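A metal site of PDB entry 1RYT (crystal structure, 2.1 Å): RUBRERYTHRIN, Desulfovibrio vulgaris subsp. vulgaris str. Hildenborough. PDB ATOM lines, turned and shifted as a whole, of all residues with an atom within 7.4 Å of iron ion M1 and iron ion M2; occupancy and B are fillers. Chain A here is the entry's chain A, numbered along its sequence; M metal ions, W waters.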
ATOM      1  N   ALA A  15     -23.805 -24.175   7.342  1.00  0.00           N
ATOM      2  CA  ALA A  15     -23.818 -22.993   6.481  1.00  0.00           C
ATOM      3  C   ALA A  15     -25.179 -22.289   6.666  1.00  0.00           C
ATOM      4  O   ALA A  15     -25.248 -21.064   6.878  1.00  0.00           O
ATOM      5  CB  ALA A  15     -23.592 -23.401   5.043  1.00  0.00           C
ATOM      6  N   GLY A  18     -25.115 -20.384  10.085  1.00  0.00           N
ATOM      7  CA  GLY A  18     -24.298 -19.186  10.071  1.00  0.00           C
ATOM      8  C   GLY A  18     -24.974 -18.144   9.205  1.00  0.00           C
ATOM      9  O   GLY A  18     -25.034 -16.964   9.585  1.00  0.00           O
ATOM     10  N   GLU A  19     -25.499 -18.538   8.050  1.00  0.00           N
ATOM     11  CA  GLU A  19     -26.166 -17.560   7.183  1.00  0.00           C
ATOM     12  C   GLU A  19     -27.397 -16.976   7.876  1.00  0.00           C
ATOM     13  O   GLU A  19     -27.678 -15.777   7.751  1.00  0.00           O
ATOM     14  CB  GLU A  19     -26.533 -18.165   5.808  1.00  0.00           C
ATOM     15  CG  GLU A  19     -25.350 -18.619   4.953  1.00  0.00           C
ATOM     16  CD  GLU A  19     -24.530 -17.471   4.354  1.00  0.00           C
ATOM     17  OE1 GLU A  19     -23.981 -16.642   5.100  1.00  0.00           O
ATOM     18  OE2 GLU A  19     -24.399 -17.415   3.115  1.00  0.00           O
ATOM     19  N   ALA A  22     -26.221 -14.395  10.253  1.00  0.00           N
ATOM     20  CA  ALA A  22     -25.681 -13.241   9.502  1.00  0.00           C
ATOM     21  C   ALA A  22     -26.809 -12.316   9.054  1.00  0.00           C
ATOM     22  O   ALA A  22     -26.684 -11.100   9.140  1.00  0.00           O
ATOM     23  CB  ALA A  22     -24.810 -13.684   8.314  1.00  0.00           C
ATOM     24  N   TYR A  26     -26.761  -8.452  10.098  1.00  0.00           N
ATOM     25  CA  TYR A  26     -26.774  -7.390   9.093  1.00  0.00           C
ATOM     26  C   TYR A  26     -27.982  -6.459   9.260  1.00  0.00           C
ATOM     27  O   TYR A  26     -27.871  -5.236   9.101  1.00  0.00           O
ATOM     28  CB  TYR A  26     -26.678  -7.950   7.649  1.00  0.00           C
ATOM     29  CG  TYR A  26     -25.353  -8.663   7.358  1.00  0.00           C
ATOM     30  CD1 TYR A  26     -24.186  -8.343   8.070  1.00  0.00           C
ATOM     31  CD2 TYR A  26     -25.290  -9.683   6.408  1.00  0.00           C
ATOM     32  CE1 TYR A  26     -22.976  -9.045   7.857  1.00  0.00           C
ATOM     33  CE2 TYR A  26     -24.078 -10.396   6.174  1.00  0.00           C
ATOM     34  CZ  TYR A  26     -22.956 -10.059   6.903  1.00  0.00           C
ATOM     35  OH  TYR A  26     -21.763 -10.739   6.676  1.00  0.00           O
ATOM     36  N   THR A  48     -27.868  -6.876   1.988  1.00  0.00           N
ATOM     37  CA  THR A  48     -27.017  -8.010   2.255  1.00  0.00           C
ATOM     38  C   THR A  48     -27.723  -9.027   3.143  1.00  0.00           C
ATOM     39  O   THR A  48     -27.606 -10.241   2.931  1.00  0.00           O
ATOM     40  CB  THR A  48     -25.693  -7.565   2.873  1.00  0.00           C
ATOM     41  OG1 THR A  48     -25.192  -6.445   2.140  1.00  0.00           O
ATOM     42  CG2 THR A  48     -24.660  -8.689   2.830  1.00  0.00           C
ATOM     43  N   GLN A  51     -29.870 -10.953   0.915  1.00  0.00           N
ATOM     44  CA  GLN A  51     -29.174 -11.886   0.062  1.00  0.00           C
ATOM     45  C   GLN A  51     -28.745 -13.100   0.860  1.00  0.00           C
ATOM     46  O   GLN A  51     -28.825 -14.210   0.339  1.00  0.00           O
ATOM     47  CB  GLN A  51     -28.002 -11.174  -0.634  1.00  0.00           C
ATOM     48  CG  GLN A  51     -28.535 -10.178  -1.643  1.00  0.00           C
ATOM     49  CD  GLN A  51     -27.453  -9.376  -2.332  1.00  0.00           C
ATOM     50  OE1 GLN A  51     -26.335  -9.260  -1.837  1.00  0.00           O
ATOM     51  NE2 GLN A  51     -27.778  -8.830  -3.483  1.00  0.00           N
ATOM     52  N   GLU A  52     -28.345 -12.943   2.118  1.00  0.00           N
ATOM     53  CA  GLU A  52     -27.986 -14.122   2.924  1.00  0.00           C
ATOM     54  C   GLU A  52     -29.215 -15.013   3.139  1.00  0.00           C
ATOM     55  O   GLU A  52     -29.112 -16.241   3.218  1.00  0.00           O
ATOM     56  CB  GLU A  52     -27.413 -13.758   4.290  1.00  0.00           C
ATOM     57  CG  GLU A  52     -26.203 -12.855   4.301  1.00  0.00           C
ATOM     58  CD  GLU A  52     -25.054 -13.307   3.401  1.00  0.00           C
ATOM     59  OE1 GLU A  52     -24.771 -14.515   3.260  1.00  0.00           O
ATOM     60  OE2 GLU A  52     -24.415 -12.408   2.823  1.00  0.00           O
ATOM     61  N   HIS A  55     -29.271 -17.190   0.164  1.00  0.00           N
ATOM     62  CA  HIS A  55     -28.222 -18.195   0.130  1.00  0.00           C
ATOM     63  C   HIS A  55     -28.740 -19.294   1.078  1.00  0.00           C
ATOM     64  O   HIS A  55     -28.683 -20.479   0.762  1.00  0.00           O
ATOM     65  CB  HIS A  55     -26.907 -17.647   0.696  1.00  0.00           C
ATOM     66  CG  HIS A  55     -26.233 -16.638  -0.186  1.00  0.00           C
ATOM     67  ND1 HIS A  55     -25.322 -15.720   0.303  1.00  0.00           N
ATOM     68  CD2 HIS A  55     -26.317 -16.412  -1.516  1.00  0.00           C
ATOM     69  CE1 HIS A  55     -24.884 -14.975  -0.694  1.00  0.00           C
ATOM     70  NE2 HIS A  55     -25.479 -15.370  -1.806  1.00  0.00           N
ATOM     71  N   ALA A  56     -29.270 -18.868   2.232  1.00  0.00           N
ATOM     72  CA  ALA A  56     -29.812 -19.793   3.213  1.00  0.00           C
ATOM     73  C   ALA A  56     -30.974 -20.642   2.657  1.00  0.00           C
ATOM     74  O   ALA A  56     -31.066 -21.837   2.926  1.00  0.00           O
ATOM     75  CB  ALA A  56     -30.212 -19.036   4.474  1.00  0.00           C
ATOM     76  N   SER A  89     -18.181  -7.285   9.754  1.00  0.00           N
ATOM     77  CA  SER A  89     -18.911  -7.951   8.681  1.00  0.00           C
ATOM     78  C   SER A  89     -17.986  -8.466   7.584  1.00  0.00           C
ATOM     79  O   SER A  89     -18.068  -9.630   7.230  1.00  0.00           O
ATOM     80  CB  SER A  89     -19.961  -6.997   8.089  1.00  0.00           C
ATOM     81  OG  SER A  89     -20.968  -6.680   9.048  1.00  0.00           O
ATOM     82  N   GLY A  92     -16.267 -11.501   8.585  1.00  0.00           N
ATOM     83  CA  GLY A  92     -17.094 -12.694   8.553  1.00  0.00           C
ATOM     84  C   GLY A  92     -17.265 -13.182   7.132  1.00  0.00           C
ATOM     85  O   GLY A  92     -17.180 -14.382   6.848  1.00  0.00           O
ATOM     86  N   GLU A  93     -17.496 -12.231   6.233  1.00  0.00           N
ATOM     87  CA  GLU A  93     -17.666 -12.506   4.810  1.00  0.00           C
ATOM     88  C   GLU A  93     -16.390 -13.126   4.321  1.00  0.00           C
ATOM     89  O   GLU A  93     -16.388 -14.131   3.610  1.00  0.00           O
ATOM     90  CB  GLU A  93     -17.911 -11.196   4.064  1.00  0.00           C
ATOM     91  CG  GLU A  93     -19.255 -10.515   4.350  1.00  0.00           C
ATOM     92  CD  GLU A  93     -20.443 -11.227   3.702  1.00  0.00           C
ATOM     93  OE1 GLU A  93     -20.216 -12.269   3.053  1.00  0.00           O
ATOM     94  OE2 GLU A  93     -21.578 -10.735   3.828  1.00  0.00           O
ATOM     95  N   HIS A  94     -15.279 -12.583   4.799  1.00  0.00           N
ATOM     96  CA  HIS A  94     -13.976 -13.053   4.401  1.00  0.00           C
ATOM     97  C   HIS A  94     -13.778 -14.514   4.693  1.00  0.00           C
ATOM     98  O   HIS A  94     -13.273 -15.254   3.847  1.00  0.00           O
ATOM     99  CB  HIS A  94     -12.874 -12.271   5.088  1.00  0.00           C
ATOM    100  CG  HIS A  94     -11.516 -12.669   4.641  1.00  0.00           C
ATOM    101  ND1 HIS A  94     -10.941 -12.173   3.482  1.00  0.00           N
ATOM    102  CD2 HIS A  94     -10.617 -13.538   5.155  1.00  0.00           C
ATOM    103  CE1 HIS A  94      -9.751 -12.719   3.315  1.00  0.00           C
ATOM    104  NE2 HIS A  94      -9.525 -13.551   4.318  1.00  0.00           N
ATOM    105  N   GLU A  96     -16.032 -16.787   5.148  1.00  0.00           N
ATOM    106  CA  GLU A  96     -16.943 -17.623   4.380  1.00  0.00           C
ATOM    107  C   GLU A  96     -16.422 -17.986   2.997  1.00  0.00           C
ATOM    108  O   GLU A  96     -16.435 -19.158   2.609  1.00  0.00           O
ATOM    109  CB  GLU A  96     -18.320 -16.956   4.277  1.00  0.00           C
ATOM    110  CG  GLU A  96     -19.198 -17.090   5.513  1.00  0.00           C
ATOM    111  CD  GLU A  96     -20.580 -16.461   5.332  1.00  0.00           C
ATOM    112  OE1 GLU A  96     -21.280 -16.780   4.362  1.00  0.00           O
ATOM    113  OE2 GLU A  96     -20.966 -15.652   6.180  1.00  0.00           O
ATOM    114  N   TYR A  97     -15.929 -17.005   2.257  1.00  0.00           N
ATOM    115  CA  TYR A  97     -15.455 -17.268   0.912  1.00  0.00           C
ATOM    116  C   TYR A  97     -14.038 -17.806   0.849  1.00  0.00           C
ATOM    117  O   TYR A  97     -13.676 -18.502  -0.084  1.00  0.00           O
ATOM    118  CB  TYR A  97     -15.675 -16.057  -0.024  1.00  0.00           C
ATOM    119  CG  TYR A  97     -14.635 -14.942  -0.002  1.00  0.00           C
ATOM    120  CD1 TYR A  97     -13.473 -15.046  -0.752  1.00  0.00           C
ATOM    121  CD2 TYR A  97     -14.837 -13.780   0.738  1.00  0.00           C
ATOM    122  CE1 TYR A  97     -12.524 -14.016  -0.772  1.00  0.00           C
ATOM    123  CE2 TYR A  97     -13.904 -12.732   0.722  1.00  0.00           C
ATOM    124  CZ  TYR A  97     -12.753 -12.865  -0.038  1.00  0.00           C
ATOM    125  OH  TYR A  97     -11.795 -11.856  -0.057  1.00  0.00           O
ATOM    126  N   MET A 100     -14.688 -21.308   4.796  1.00  0.00           N
ATOM    127  CA  MET A 100     -15.869 -22.171   4.878  1.00  0.00           C
ATOM    128  C   MET A 100     -16.336 -22.779   3.559  1.00  0.00           C
ATOM    129  O   MET A 100     -16.248 -23.994   3.359  1.00  0.00           O
ATOM    130  CB  MET A 100     -17.012 -21.416   5.546  1.00  0.00           C
ATOM    131  CG  MET A 100     -18.145 -22.329   5.987  1.00  0.00           C
ATOM    132  SD  MET A 100     -19.504 -21.396   6.671  1.00  0.00           S
ATOM    133  CE  MET A 100     -20.402 -21.115   5.224  1.00  0.00           C
ATOM    134  N   TYR A 101     -16.830 -21.947   2.648  1.00  0.00           N
ATOM    135  CA  TYR A 101     -17.324 -22.445   1.379  1.00  0.00           C
ATOM    136  C   TYR A 101     -16.381 -23.301   0.513  1.00  0.00           C
ATOM    137  O   TYR A 101     -16.803 -24.335  -0.016  1.00  0.00           O
ATOM    138  CB  TYR A 101     -17.981 -21.317   0.580  1.00  0.00           C
ATOM    139  CG  TYR A 101     -19.358 -20.930   1.102  1.00  0.00           C
ATOM    140  CD1 TYR A 101     -20.398 -21.867   1.113  1.00  0.00           C
ATOM    141  CD2 TYR A 101     -19.607 -19.646   1.573  1.00  0.00           C
ATOM    142  CE1 TYR A 101     -21.674 -21.521   1.576  1.00  0.00           C
ATOM    143  CE2 TYR A 101     -20.872 -19.293   2.054  1.00  0.00           C
ATOM    144  CZ  TYR A 101     -21.894 -20.235   2.034  1.00  0.00           C
ATOM    145  OH  TYR A 101     -23.179 -19.870   2.425  1.00  0.00           O
ATOM    146  N   ILE A 123     -21.754 -19.387  -4.241  1.00  0.00           N
ATOM    147  CA  ILE A 123     -22.112 -18.495  -3.139  1.00  0.00           C
ATOM    148  C   ILE A 123     -20.880 -17.697  -2.706  1.00  0.00           C
ATOM    149  O   ILE A 123     -20.973 -16.496  -2.433  1.00  0.00           O
ATOM    150  CB  ILE A 123     -22.703 -19.290  -1.933  1.00  0.00           C
ATOM    151  CG1 ILE A 123     -24.074 -19.865  -2.308  1.00  0.00           C
ATOM    152  CG2 ILE A 123     -22.820 -18.409  -0.701  1.00  0.00           C
ATOM    153  CD1 ILE A 123     -24.587 -20.930  -1.336  1.00  0.00           C
ATOM    154  N   ALA A 126     -20.309 -14.434  -4.427  1.00  0.00           N
ATOM    155  CA  ALA A 126     -21.152 -13.340  -3.928  1.00  0.00           C
ATOM    156  C   ALA A 126     -20.618 -12.834  -2.582  1.00  0.00           C
ATOM    157  O   ALA A 126     -20.686 -11.634  -2.275  1.00  0.00           O
ATOM    158  CB  ALA A 126     -22.582 -13.838  -3.764  1.00  0.00           C
ATOM    159  N   GLU A 127     -20.076 -13.754  -1.806  1.00  0.00           N
ATOM    160  CA  GLU A 127     -19.523 -13.434  -0.507  1.00  0.00           C
ATOM    161  C   GLU A 127     -18.271 -12.590  -0.643  1.00  0.00           C
ATOM    162  O   GLU A 127     -17.907 -11.852   0.264  1.00  0.00           O
ATOM    163  CB  GLU A 127     -19.279 -14.698   0.312  1.00  0.00           C
ATOM    164  CG  GLU A 127     -20.462 -15.652   0.366  1.00  0.00           C
ATOM    165  CD  GLU A 127     -21.646 -15.148   1.189  1.00  0.00           C
ATOM    166  OE1 GLU A 127     -21.974 -13.944   1.179  1.00  0.00           O
ATOM    167  OE2 GLU A 127     -22.298 -15.989   1.831  1.00  0.00           O
ATOM    168  N   GLU A 128     -17.607 -12.687  -1.789  1.00  0.00           N
ATOM    169  CA  GLU A 128     -16.413 -11.881  -2.023  1.00  0.00           C
ATOM    170  C   GLU A 128     -16.775 -10.416  -2.326  1.00  0.00           C
ATOM    171  O   GLU A 128     -16.094  -9.504  -1.870  1.00  0.00           O
ATOM    172  CB  GLU A 128     -15.557 -12.488  -3.134  1.00  0.00           C
ATOM    173  CG  GLU A 128     -14.347 -11.662  -3.495  1.00  0.00           C
ATOM    174  CD  GLU A 128     -13.268 -12.494  -4.179  1.00  0.00           C
ATOM    175  OE1 GLU A 128     -13.604 -13.538  -4.790  1.00  0.00           O
ATOM    176  OE2 GLU A 128     -12.080 -12.113  -4.079  1.00  0.00           O
ATOM    177  N   PHE A 129     -17.862 -10.191  -3.072  1.00  0.00           N
ATOM    178  CA  PHE A 129     -18.286  -8.808  -3.357  1.00  0.00           C
ATOM    179  C   PHE A 129     -18.855  -8.143  -2.071  1.00  0.00           C
ATOM    180  O   PHE A 129     -18.620  -6.955  -1.829  1.00  0.00           O
ATOM    181  CB  PHE A 129     -19.280  -8.744  -4.547  1.00  0.00           C
ATOM    182  CG  PHE A 129     -19.690  -7.330  -4.939  1.00  0.00           C
ATOM    183  CD1 PHE A 129     -18.730  -6.388  -5.340  1.00  0.00           C
ATOM    184  CD2 PHE A 129     -21.020  -6.907  -4.830  1.00  0.00           C
ATOM    185  CE1 PHE A 129     -19.083  -5.044  -5.617  1.00  0.00           C
ATOM    186  CE2 PHE A 129     -21.381  -5.565  -5.102  1.00  0.00           C
ATOM    187  CZ  PHE A 129     -20.409  -4.637  -5.493  1.00  0.00           C
ATOM    188  N   HIS A 130     -19.542  -8.898  -1.224  1.00  0.00           N
ATOM    189  CA  HIS A 130     -20.080  -8.336   0.019  1.00  0.00           C
ATOM    190  C   HIS A 130     -18.978  -7.768   0.867  1.00  0.00           C
ATOM    191  O   HIS A 130     -19.139  -6.702   1.424  1.00  0.00           O
ATOM    192  CB  HIS A 130     -20.783  -9.404   0.869  1.00  0.00           C
ATOM    193  CG  HIS A 130     -22.068  -9.895   0.265  1.00  0.00           C
ATOM    194  ND1 HIS A 130     -22.699 -11.031   0.705  1.00  0.00           N
ATOM    195  CD2 HIS A 130     -22.867  -9.375  -0.703  1.00  0.00           C
ATOM    196  CE1 HIS A 130     -23.833 -11.192   0.044  1.00  0.00           C
ATOM    197  NE2 HIS A 130     -23.960 -10.204  -0.817  1.00  0.00           N
ATOM    198  N   GLU A 131     -17.884  -8.516   1.001  1.00  0.00           N
ATOM    199  CA  GLU A 131     -16.725  -8.081   1.794  1.00  0.00           C
ATOM    200  C   GLU A 131     -16.104  -6.839   1.214  1.00  0.00           C
ATOM    201  O   GLU A 131     -15.799  -5.901   1.924  1.00  0.00           O
ATOM    202  CB  GLU A 131     -15.640  -9.134   1.820  1.00  0.00           C
ATOM    203  CG  GLU A 131     -14.485  -8.680   2.669  1.00  0.00           C
ATOM    204  CD  GLU A 131     -13.159  -9.319   2.292  1.00  0.00           C
ATOM    205  OE1 GLU A 131     -12.954  -9.631   1.100  1.00  0.00           O
ATOM    206  OE2 GLU A 131     -12.318  -9.472   3.195  1.00  0.00           O
ATOM    207  N   PHE A 134     -18.207  -3.828   1.897  1.00  0.00           N
ATOM    208  CA  PHE A 134     -18.145  -3.420   3.307  1.00  0.00           C
ATOM    209  C   PHE A 134     -16.842  -2.718   3.631  1.00  0.00           C
ATOM    210  O   PHE A 134     -16.792  -1.801   4.476  1.00  0.00           O
ATOM    211  CB  PHE A 134     -18.326  -4.631   4.257  1.00  0.00           C
ATOM    212  CG  PHE A 134     -19.745  -5.140   4.342  1.00  0.00           C
ATOM    213  CD1 PHE A 134     -20.840  -4.254   4.291  1.00  0.00           C
ATOM    214  CD2 PHE A 134     -19.991  -6.491   4.518  1.00  0.00           C
ATOM    215  CE1 PHE A 134     -22.130  -4.722   4.414  1.00  0.00           C
ATOM    216  CE2 PHE A 134     -21.303  -6.977   4.639  1.00  0.00           C
ATOM    217  CZ  PHE A 134     -22.366  -6.083   4.582  1.00  0.00           C
HETATM  218 FE    FE M   1     -22.915 -15.491   3.712  1.00  0.00          FE
HETATM  219 FE    FE M   2     -22.304 -12.556   2.646  1.00  0.00          FE
HETATM  220  O   HOH W   1     -22.143 -13.866   4.387  1.00  0.00           O
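Iron ion M2 is bound by the side-chain carboxylate (OE1) of Glu 127.
OE2 of Glu 52 binds iron ion M2, 2.1 Å away.
OE1 of Glu 93 is bound to iron ion M2 (2.1 Å).
Water W1 is bound to iron ion M2 (2.2 Å).
OE2 of Glu 93 is bound to iron ion M2 (2.3 Å).
Iron ion M2 is bound by ND1 of His 130 (2.5 Å).
Iron ion M2 has six donor atoms within binding distance.
The nearest printed residue that does not touch iron ion M2 is Tyr 26 (4.5 Å).
Iron ion M1 is bound by water W1 (1.9 Å), the side-chain carboxylate (OE2) of Glu 127 (2.0 Å), the side-chain carboxylate (OE1) of Glu 19 (2.1 Å), the side-chain carboxylate (OE1) of Glu 52 (2.1 Å), the side-chain carboxylate (OE1) of Glu 96 (2.2 Å) and the side-chain carboxylate (OE2) of Glu 19 (2.5 Å).
Iron ion M1 has six donor atoms within binding distance.
OE2 of Glu 127 lies close to ND1 of His 55, 3.4 Å away.
ND1 of His 55 lies close to OE2 of Glu 19, 3.4 Å away.
OE2 of Glu 19 lies close to OH of Tyr 101, 2.8 Å away.
ND1 of His 55 lies close to OE1 of Glu 52, 3.2 Å away.
The side-chain hydroxyl (OH) of Tyr 26 sits close to the side-chain carboxylate (OE2) of Glu 93 (2.9 Å).
O of Glu 96 lies within hydrogen-bond range of N of Tyr 101, 2.8 Å away.
OE1 of Gln 51 sits at hydrogen-bond distance from NE2 of His 130 (2.8 Å).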
